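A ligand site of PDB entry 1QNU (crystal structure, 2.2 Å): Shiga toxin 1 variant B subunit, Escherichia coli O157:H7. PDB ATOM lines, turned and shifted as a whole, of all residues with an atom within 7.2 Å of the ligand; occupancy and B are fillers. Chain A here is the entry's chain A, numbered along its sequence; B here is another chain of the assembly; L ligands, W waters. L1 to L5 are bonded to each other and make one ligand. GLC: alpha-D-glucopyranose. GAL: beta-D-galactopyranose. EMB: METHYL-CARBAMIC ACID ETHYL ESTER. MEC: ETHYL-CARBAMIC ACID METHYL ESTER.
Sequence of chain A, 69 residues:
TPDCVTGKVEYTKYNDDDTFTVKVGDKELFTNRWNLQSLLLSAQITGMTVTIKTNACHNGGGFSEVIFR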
ATOM      1  N   THR A   1      23.091  27.087 -12.663  1.00  0.00           N
ATOM      2  CA  THR A   1      23.387  26.022 -11.646  1.00  0.00           C
ATOM      3  C   THR A   1      23.502  26.685 -10.278  1.00  0.00           C
ATOM      4  O   THR A   1      24.192  27.705 -10.129  1.00  0.00           O
ATOM      5  CB  THR A   1      24.720  25.305 -11.957  1.00  0.00           C
ATOM      6  OG1 THR A   1      24.727  24.910 -13.338  1.00  0.00           O
ATOM      7  CG2 THR A   1      24.904  24.078 -11.076  1.00  0.00           C
ATOM      8  N   PRO A   2      22.842  26.124  -9.251  1.00  0.00           N
ATOM      9  CA  PRO A   2      22.902  26.715  -7.911  1.00  0.00           C
ATOM     10  C   PRO A   2      24.245  26.538  -7.189  1.00  0.00           C
ATOM     11  O   PRO A   2      24.967  25.556  -7.400  1.00  0.00           O
ATOM     12  CB  PRO A   2      21.772  26.009  -7.176  1.00  0.00           C
ATOM     13  CG  PRO A   2      21.779  24.645  -7.800  1.00  0.00           C
ATOM     14  CD  PRO A   2      21.946  24.957  -9.283  1.00  0.00           C
ATOM     15  N   THR A  19      40.110  11.208 -11.749  1.00  0.00           N
ATOM     16  CA  THR A  19      39.215  12.314 -11.423  1.00  0.00           C
ATOM     17  C   THR A  19      39.918  13.026 -10.277  1.00  0.00           C
ATOM     18  O   THR A  19      40.919  12.523  -9.758  1.00  0.00           O
ATOM     19  CB  THR A  19      37.773  11.870 -10.990  1.00  0.00           C
ATOM     20  OG1 THR A  19      37.850  11.013  -9.847  1.00  0.00           O
ATOM     21  CG2 THR A  19      37.064  11.175 -12.138  1.00  0.00           C
ATOM     22  N   PHE A  30      33.829  15.841  -6.443  1.00  0.00           N
ATOM     23  CA  PHE A  30      34.815  15.465  -7.437  1.00  0.00           C
ATOM     24  C   PHE A  30      34.460  16.038  -8.811  1.00  0.00           C
ATOM     25  O   PHE A  30      33.310  16.366  -9.070  1.00  0.00           O
ATOM     26  CB  PHE A  30      34.912  13.936  -7.578  1.00  0.00           C
ATOM     27  CG  PHE A  30      33.819  13.334  -8.444  1.00  0.00           C
ATOM     28  CD1 PHE A  30      32.591  12.968  -7.900  1.00  0.00           C
ATOM     29  CD2 PHE A  30      34.024  13.127  -9.812  1.00  0.00           C
ATOM     30  CE1 PHE A  30      31.582  12.428  -8.700  1.00  0.00           C
ATOM     31  CE2 PHE A  30      33.019  12.587 -10.626  1.00  0.00           C
ATOM     32  CZ  PHE A  30      31.801  12.233 -10.065  1.00  0.00           C
ATOM     33  N   THR A  31      35.465  16.144  -9.680  1.00  0.00           N
ATOM     34  CA  THR A  31      35.269  16.607 -11.040  1.00  0.00           C
ATOM     35  C   THR A  31      36.087  15.741 -11.995  1.00  0.00           C
ATOM     36  O   THR A  31      37.189  15.283 -11.663  1.00  0.00           O
ATOM     37  CB  THR A  31      35.669  18.081 -11.231  1.00  0.00           C
ATOM     38  OG1 THR A  31      35.388  18.486 -12.576  1.00  0.00           O
ATOM     39  CG2 THR A  31      37.176  18.292 -10.913  1.00  0.00           C
ATOM     40  N   ASN A  32      35.539  15.509 -13.183  1.00  0.00           N
ATOM     41  CA  ASN A  32      36.223  14.717 -14.203  1.00  0.00           C
ATOM     42  C   ASN A  32      36.856  15.609 -15.267  1.00  0.00           C
ATOM     43  O   ASN A  32      37.298  15.109 -16.288  1.00  0.00           O
ATOM     44  CB  ASN A  32      35.257  13.737 -14.868  1.00  0.00           C
ATOM     45  CG  ASN A  32      34.105  14.434 -15.602  1.00  0.00           C
ATOM     46  OD1 ASN A  32      34.078  15.661 -15.752  1.00  0.00           O
ATOM     47  ND2 ASN A  32      33.149  13.635 -16.065  1.00  0.00           N
ATOM     48  N   ARG A  33      36.875  16.930 -15.054  1.00  0.00           N
ATOM     49  CA  ARG A  33      37.475  17.835 -16.032  1.00  0.00           C
ATOM     50  C   ARG A  33      38.965  17.956 -15.737  1.00  0.00           C
ATOM     51  O   ARG A  33      39.362  18.467 -14.693  1.00  0.00           O
ATOM     52  CB  ARG A  33      36.796  19.222 -15.988  1.00  0.00           C
ATOM     53  CG  ARG A  33      35.272  19.185 -16.127  1.00  0.00           C
ATOM     54  CD  ARG A  33      34.850  18.521 -17.444  1.00  0.00           C
ATOM     55  NE  ARG A  33      33.399  18.353 -17.518  1.00  0.00           N
ATOM     56  CZ  ARG A  33      32.528  19.245 -18.002  1.00  0.00           C
ATOM     57  NH1 ARG A  33      32.940  20.411 -18.479  1.00  0.00           N
ATOM     58  NH2 ARG A  33      31.226  18.977 -18.015  1.00  0.00           N
ATOM     59  N   LEU A  36      40.649  21.392 -14.742  1.00  0.00           N
ATOM     60  CA  LEU A  36      40.451  21.889 -13.384  1.00  0.00           C
ATOM     61  C   LEU A  36      41.452  21.397 -12.320  1.00  0.00           C
ATOM     62  O   LEU A  36      41.546  21.981 -11.243  1.00  0.00           O
ATOM     63  CB  LEU A  36      39.030  21.563 -12.913  1.00  0.00           C
ATOM     64  CG  LEU A  36      37.917  22.477 -13.439  1.00  0.00           C
ATOM     65  CD1 LEU A  36      36.581  21.875 -13.071  1.00  0.00           C
ATOM     66  CD2 LEU A  36      38.068  23.888 -12.830  1.00  0.00           C
ATOM     67  N   LYS A  53      29.536  25.320  -8.001  1.00  0.00           N
ATOM     68  CA  LYS A  53      28.134  25.251  -8.361  1.00  0.00           C
ATOM     69  C   LYS A  53      27.800  23.865  -8.913  1.00  0.00           C
ATOM     70  O   LYS A  53      28.415  23.412  -9.894  1.00  0.00           O
ATOM     71  CB  LYS A  53      27.810  26.303  -9.437  1.00  0.00           C
ATOM     72  CG  LYS A  53      28.025  27.731  -8.988  1.00  0.00           C
ATOM     73  CD  LYS A  53      28.007  28.683 -10.169  1.00  0.00           C
ATOM     74  CE  LYS A  53      26.636  29.269 -10.424  1.00  0.00           C
ATOM     75  NZ  LYS A  53      26.128  30.016  -9.241  1.00  0.00           N
ATOM     76  N   THR A  54      26.834  23.186  -8.302  1.00  0.00           N
ATOM     77  CA  THR A  54      26.418  21.878  -8.764  1.00  0.00           C
ATOM     78  C   THR A  54      25.060  21.479  -8.175  1.00  0.00           C
ATOM     79  O   THR A  54      24.737  21.879  -7.063  1.00  0.00           O
ATOM     80  CB  THR A  54      27.441  20.781  -8.396  1.00  0.00           C
ATOM     81  OG1 THR A  54      26.964  19.518  -8.863  1.00  0.00           O
ATOM     82  CG2 THR A  54      27.647  20.697  -6.866  1.00  0.00           C
ATOM     83  N   ASN A  55      24.289  20.692  -8.917  1.00  0.00           N
ATOM     84  CA  ASN A  55      22.990  20.202  -8.463  1.00  0.00           C
ATOM     85  C   ASN A  55      23.179  18.965  -7.572  1.00  0.00           C
ATOM     86  O   ASN A  55      22.267  18.576  -6.840  1.00  0.00           O
ATOM     87  CB  ASN A  55      22.105  19.833  -9.661  1.00  0.00           C
ATOM     88  CG  ASN A  55      21.393  21.030 -10.252  1.00  0.00           C
ATOM     89  OD1 ASN A  55      21.292  21.164 -11.474  1.00  0.00           O
ATOM     90  ND2 ASN A  55      20.890  21.904  -9.398  1.00  0.00           N
ATOM     91  N   ALA A  56      24.363  18.360  -7.644  1.00  0.00           N
ATOM     92  CA  ALA A  56      24.670  17.190  -6.833  1.00  0.00           C
ATOM     93  C   ALA A  56      25.431  17.672  -5.624  1.00  0.00           C
ATOM     94  O   ALA A  56      26.575  17.272  -5.377  1.00  0.00           O
ATOM     95  CB  ALA A  56      25.538  16.203  -7.636  1.00  0.00           C
ATOM     96  N   CYS A  57      24.790  18.541  -4.853  1.00  0.00           N
ATOM     97  CA  CYS A  57      25.412  19.135  -3.689  1.00  0.00           C
ATOM     98  C   CYS A  57      25.377  18.261  -2.444  1.00  0.00           C
ATOM     99  O   CYS A  57      24.656  18.530  -1.494  1.00  0.00           O
ATOM    100  CB  CYS A  57      24.780  20.508  -3.387  1.00  0.00           C
ATOM    101  SG  CYS A  57      25.704  21.518  -2.197  1.00  0.00           S
ATOM    102  N   HIS A  58      26.193  17.202  -2.463  1.00  0.00           N
ATOM    103  CA  HIS A  58      26.288  16.262  -1.348  1.00  0.00           C
ATOM    104  C   HIS A  58      27.663  15.586  -1.472  1.00  0.00           C
ATOM    105  O   HIS A  58      28.261  15.601  -2.544  1.00  0.00           O
ATOM    106  CB  HIS A  58      25.162  15.217  -1.438  1.00  0.00           C
ATOM    107  CG  HIS A  58      25.116  14.497  -2.761  1.00  0.00           C
ATOM    108  ND1 HIS A  58      25.981  13.458  -3.069  1.00  0.00           N
ATOM    109  CD2 HIS A  58      24.353  14.686  -3.853  1.00  0.00           C
ATOM    110  CE1 HIS A  58      25.738  13.052  -4.315  1.00  0.00           C
ATOM    111  NE2 HIS A  58      24.760  13.782  -4.808  1.00  0.00           N
ATOM    112  N   GLY A  60      30.549  13.323  -2.289  1.00  0.00           N
ATOM    113  CA  GLY A  60      30.663  12.393  -3.409  1.00  0.00           C
ATOM    114  C   GLY A  60      30.054  12.920  -4.699  1.00  0.00           C
ATOM    115  O   GLY A  60      30.244  12.327  -5.761  1.00  0.00           O
ATOM    116  N   GLY A  61      29.313  14.030  -4.631  1.00  0.00           N
ATOM    117  CA  GLY A  61      28.710  14.590  -5.841  1.00  0.00           C
ATOM    118  C   GLY A  61      29.725  15.172  -6.810  1.00  0.00           C
ATOM    119  O   GLY A  61      30.820  15.571  -6.421  1.00  0.00           O
ATOM    120  N   GLY A  62      29.384  15.232  -8.090  1.00  0.00           N
ATOM    121  CA  GLY A  62      30.322  15.770  -9.058  1.00  0.00           C
ATOM    122  C   GLY A  62      30.030  17.213  -9.419  1.00  0.00           C
ATOM    123  O   GLY A  62      28.947  17.726  -9.122  1.00  0.00           O
ATOM    124  N   PHE A  63      30.992  17.886 -10.024  1.00  0.00           N
ATOM    125  CA  PHE A  63      30.800  19.268 -10.450  1.00  0.00           C
ATOM    126  C   PHE A  63      31.717  19.577 -11.627  1.00  0.00           C
ATOM    127  O   PHE A  63      32.664  18.829 -11.901  1.00  0.00           O
ATOM    128  CB  PHE A  63      31.118  20.259  -9.310  1.00  0.00           C
ATOM    129  CG  PHE A  63      32.585  20.341  -8.976  1.00  0.00           C
ATOM    130  CD1 PHE A  63      33.192  19.404  -8.125  1.00  0.00           C
ATOM    131  CD2 PHE A  63      33.385  21.326  -9.546  1.00  0.00           C
ATOM    132  CE1 PHE A  63      34.560  19.449  -7.855  1.00  0.00           C
ATOM    133  CE2 PHE A  63      34.770  21.381  -9.286  1.00  0.00           C
ATOM    134  CZ  PHE A  63      35.346  20.445  -8.437  1.00  0.00           C
ATOM    135  N   SER A  64      31.425  20.673 -12.305  1.00  0.00           N
ATOM    136  CA  SER A  64      32.254  21.148 -13.397  1.00  0.00           C
ATOM    137  C   SER A  64      32.379  22.678 -13.309  1.00  0.00           C
ATOM    138  O   SER A  64      33.290  23.254 -13.903  1.00  0.00           O
ATOM    139  CB  SER A  64      31.654  20.781 -14.749  1.00  0.00           C
ATOM    140  OG  SER A  64      30.400  21.392 -14.941  1.00  0.00           O
ATOM    141  N   GLU A  65      31.481  23.331 -12.567  1.00  0.00           N
ATOM    142  CA  GLU A  65      31.508  24.799 -12.461  1.00  0.00           C
ATOM    143  C   GLU A  65      32.090  25.326 -11.188  1.00  0.00           C
ATOM    144  O   GLU A  65      31.621  24.983 -10.093  1.00  0.00           O
ATOM    145  CB  GLU A  65      30.093  25.364 -12.624  1.00  0.00           C
ATOM    146  CG  GLU A  65      29.474  25.031 -13.954  1.00  0.00           C
ATOM    147  CD  GLU A  65      28.064  25.587 -14.108  1.00  0.00           C
ATOM    148  OE1 GLU A  65      27.895  26.821 -13.997  1.00  0.00           O
ATOM    149  OE2 GLU A  65      27.140  24.800 -14.342  1.00  0.00           O
ATOM    150  N   ASP B  16      30.475  24.814 -17.604  1.00  0.00           N
ATOM    151  CA  ASP B  16      30.108  23.427 -17.871  1.00  0.00           C
ATOM    152  C   ASP B  16      30.481  22.958 -19.282  1.00  0.00           C
ATOM    153  O   ASP B  16      30.715  21.761 -19.501  1.00  0.00           O
ATOM    154  CB  ASP B  16      28.619  23.243 -17.617  1.00  0.00           C
ATOM    155  CG  ASP B  16      28.185  21.780 -17.694  1.00  0.00           C
ATOM    156  OD1 ASP B  16      28.587  20.985 -16.820  1.00  0.00           O
ATOM    157  OD2 ASP B  16      27.435  21.447 -18.627  1.00  0.00           O
ATOM    158  N   ASP B  18      33.181  23.783 -20.775  1.00  0.00           N
ATOM    159  CA  ASP B  18      34.641  23.924 -20.828  1.00  0.00           C
ATOM    160  C   ASP B  18      35.180  25.276 -21.306  1.00  0.00           C
ATOM    161  O   ASP B  18      36.357  25.377 -21.639  1.00  0.00           O
ATOM    162  CB  ASP B  18      35.265  22.805 -21.660  1.00  0.00           C
ATOM    163  CG  ASP B  18      35.016  21.424 -21.060  1.00  0.00           C
ATOM    164  OD1 ASP B  18      35.395  21.181 -19.892  1.00  0.00           O
ATOM    165  OD2 ASP B  18      34.438  20.591 -21.766  1.00  0.00           O
HETATM  166  C1  GLC L   1      19.226  16.093 -12.840  1.00  0.00           C
HETATM  167  C2  GLC L   1      20.019  17.357 -13.166  1.00  0.00           C
HETATM  168  C3  GLC L   1      21.498  17.001 -13.414  1.00  0.00           C
HETATM  169  C4  GLC L   1      22.063  16.161 -12.262  1.00  0.00           C
HETATM  170  C5  GLC L   1      21.142  14.969 -11.984  1.00  0.00           C
HETATM  171  C6  GLC L   1      21.578  14.140 -10.789  1.00  0.00           C
HETATM  172  O1  GLC L   1      17.922  16.428 -12.511  1.00  0.00           O
HETATM  173  O2  GLC L   1      19.477  17.964 -14.323  1.00  0.00           O
HETATM  174  O3  GLC L   1      22.254  18.202 -13.534  1.00  0.00           O
HETATM  175  O4  GLC L   1      23.370  15.680 -12.628  1.00  0.00           O
HETATM  176  O5  GLC L   1      19.805  15.440 -11.707  1.00  0.00           O
HETATM  177  O6  GLC L   1      22.206  14.950  -9.802  1.00  0.00           O
HETATM  178  C1  GAL L   2      24.445  16.137 -11.871  1.00  0.00           C
HETATM  179  C2  GAL L   2      25.623  15.163 -12.010  1.00  0.00           C
HETATM  180  C3  GAL L   2      26.885  15.727 -11.344  1.00  0.00           C
HETATM  181  C4  GAL L   2      27.163  17.148 -11.826  1.00  0.00           C
HETATM  182  C5  GAL L   2      25.909  18.010 -11.646  1.00  0.00           C
HETATM  183  C6  GAL L   2      26.071  19.440 -12.126  1.00  0.00           C
HETATM  184  O2  GAL L   2      25.272  13.910 -11.386  1.00  0.00           O
HETATM  185  O3  GAL L   2      27.997  14.892 -11.640  1.00  0.00           O
HETATM  186  O4  GAL L   2      27.554  17.120 -13.215  1.00  0.00           O
HETATM  187  O5  GAL L   2      24.816  17.432 -12.380  1.00  0.00           O
HETATM  188  O6  GAL L   2      24.993  20.260 -11.672  1.00  0.00           O
HETATM  189  C1  GAL L   3      28.703  17.858 -13.555  1.00  0.00           C
HETATM  190  C2  GAL L   3      28.801  18.036 -15.074  1.00  0.00           C
HETATM  191  C3  GAL L   3      29.047  16.698 -15.748  1.00  0.00           C
HETATM  192  C4  GAL L   3      30.326  16.083 -15.180  1.00  0.00           C
HETATM  193  C5  GAL L   3      30.207  15.954 -13.654  1.00  0.00           C
HETATM  194  C6  GAL L   3      31.475  15.441 -12.990  1.00  0.00           C
HETATM  195  O2  GAL L   3      27.603  18.621 -15.580  1.00  0.00           O
HETATM  196  O3  GAL L   3      29.173  16.873 -17.148  1.00  0.00           O
HETATM  197  O4  GAL L   3      31.434  16.912 -15.513  1.00  0.00           O
HETATM  198  O5  GAL L   3      29.894  17.239 -13.056  1.00  0.00           O
HETATM  199  O6  GAL L   3      32.531  16.386 -13.086  1.00  0.00           O
HETATM  200  C1  EMB L   4      24.595  12.824 -12.066  1.00  0.00           C
HETATM  201  C2  EMB L   4      25.684  11.822 -12.436  1.00  0.00           C
HETATM  202  O1  EMB L   4      26.527  12.338 -13.540  1.00  0.00           O
HETATM  203  C3  EMB L   4      27.795  11.925 -13.463  1.00  0.00           C
HETATM  204  O2  EMB L   4      28.255  11.004 -12.788  1.00  0.00           O
HETATM  205  N1  EMB L   4      28.461  12.471 -14.487  1.00  0.00           N
HETATM  206  C4  EMB L   4      29.839  12.153 -14.832  1.00  0.00           C
HETATM  207  C2  MEC L   5      29.549  11.721 -16.268  1.00  0.00           C
HETATM  208  O1  MEC L   5      29.639  13.072 -16.869  1.00  0.00           O
HETATM  209  C3  MEC L   5      29.893  13.056 -18.187  1.00  0.00           C
HETATM  210  O2  MEC L   5      30.375  12.152 -18.855  1.00  0.00           O
HETATM  211  N1  MEC L   5      29.749  14.295 -18.652  1.00  0.00           N
HETATM  212  C4  MEC L   5      30.099  14.709 -20.005  1.00  0.00           C
HETATM  213  C5  MEC L   5      31.255  15.705 -20.023  1.00  0.00           C
HETATM  214  O   HOH W   1      24.344  21.351 -13.964  1.00  0.00           O
HETATM  215  O   HOH W   2      25.001  17.358 -15.382  1.00  0.00           O
HETATM  216  O   HOH W   3      27.378  13.046  -9.064  1.00  0.00           O
HETATM  217  O   HOH W   4      28.749  21.654 -11.850  1.00  0.00           O
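The side-chain carboxylate of Asp 16 of chain B is in hydrogen-bond range of an oxygen (O2) of GAL L3 (2.8 Å).
An oxygen (O4) of GAL L3 sits at hydrogen-bond distance from the side-chain amide oxygen (OD1) of Asn 32.
An oxygen (O3) of GAL L3 sits at hydrogen-bond distance from the guanidinium group of Arg 33 (3.1 Å).
The backbone NH (N) of Asn 32 is in hydrogen-bond range of an oxygen (O6) of GAL L3, at 3.1 Å.
The backbone NH of Phe 63 is in hydrogen-bond range of an oxygen (O5) of GAL L3, at 3.3 Å.
The backbone NH of Asn 55 lies within hydrogen-bond range of an oxygen (O6) of GAL L2 (2.9 Å).
The backbone carbonyl oxygen (O) of Phe 63 lies within hydrogen-bond range of an oxygen (O6) of GAL L3 (2.7 Å).
The guanidinium group of Arg 33 is in salt-bridge range of the side-chain carboxylate of Asp 16 of chain B.
The backbone NH (N) of Phe 63 lies within hydrogen-bond range of the backbone carbonyl oxygen (O) of Phe 30, 2.9 Å away.
The side-chain hydroxyl (OG1) of Thr 31 sits at hydrogen-bond distance from the backbone NH (N) of Arg 33 (3.3 Å).
OG1 of Thr 54 sits at hydrogen-bond distance from N of Ala 56 (3.1 Å).
NZ of Lys 53 sits close to O of Thr 1.
The side-chain amide oxygen (OD1) of Asn 32 is in hydrogen-bond range of the guanidinium group (NE) of Arg 33 (3.3 Å).
NH1 of Arg 33 lies within salt-bridge range of OD1 of Asp 18 of chain B, 2.9 Å away.
The backbone NH (N) of Thr 54 sits at hydrogen-bond distance from the backbone carbonyl oxygen (O) of Pro 2 (3.1 Å).
Thr 1 touches the ligand.
CA of Thr 31 touches O6 of GAL L3, at 3.4 Å.
OG1 of Thr 54 touches C5 of GAL L2, at 3.3 Å.
Ala 56 touches the ligand.
O of Gly 62 touches C4 of GAL L2 (3.3 Å).
Ser 64 touches the ligand.
11 residues have an atom within 4 Å of the ligand: Thr 1, Thr 31, Asn 32, Arg 33, Thr 54, Asn 55, Ala 56, Gly 62, Phe 63, Ser 64 and Asp 16 of chain B.
Water W3 bridges the backbone NH of Gly 62 (3.1 Å) and an oxygen (O3) of GAL L2 (3.2 Å).
Water W4 lies within hydrogen-bond range of the backbone carbonyl oxygen (O) of Lys 53 (2.7 Å), the backbone NH (N) of Ser 64 (2.9 Å) and the backbone NH (N) of Glu 65 (3.3 Å).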
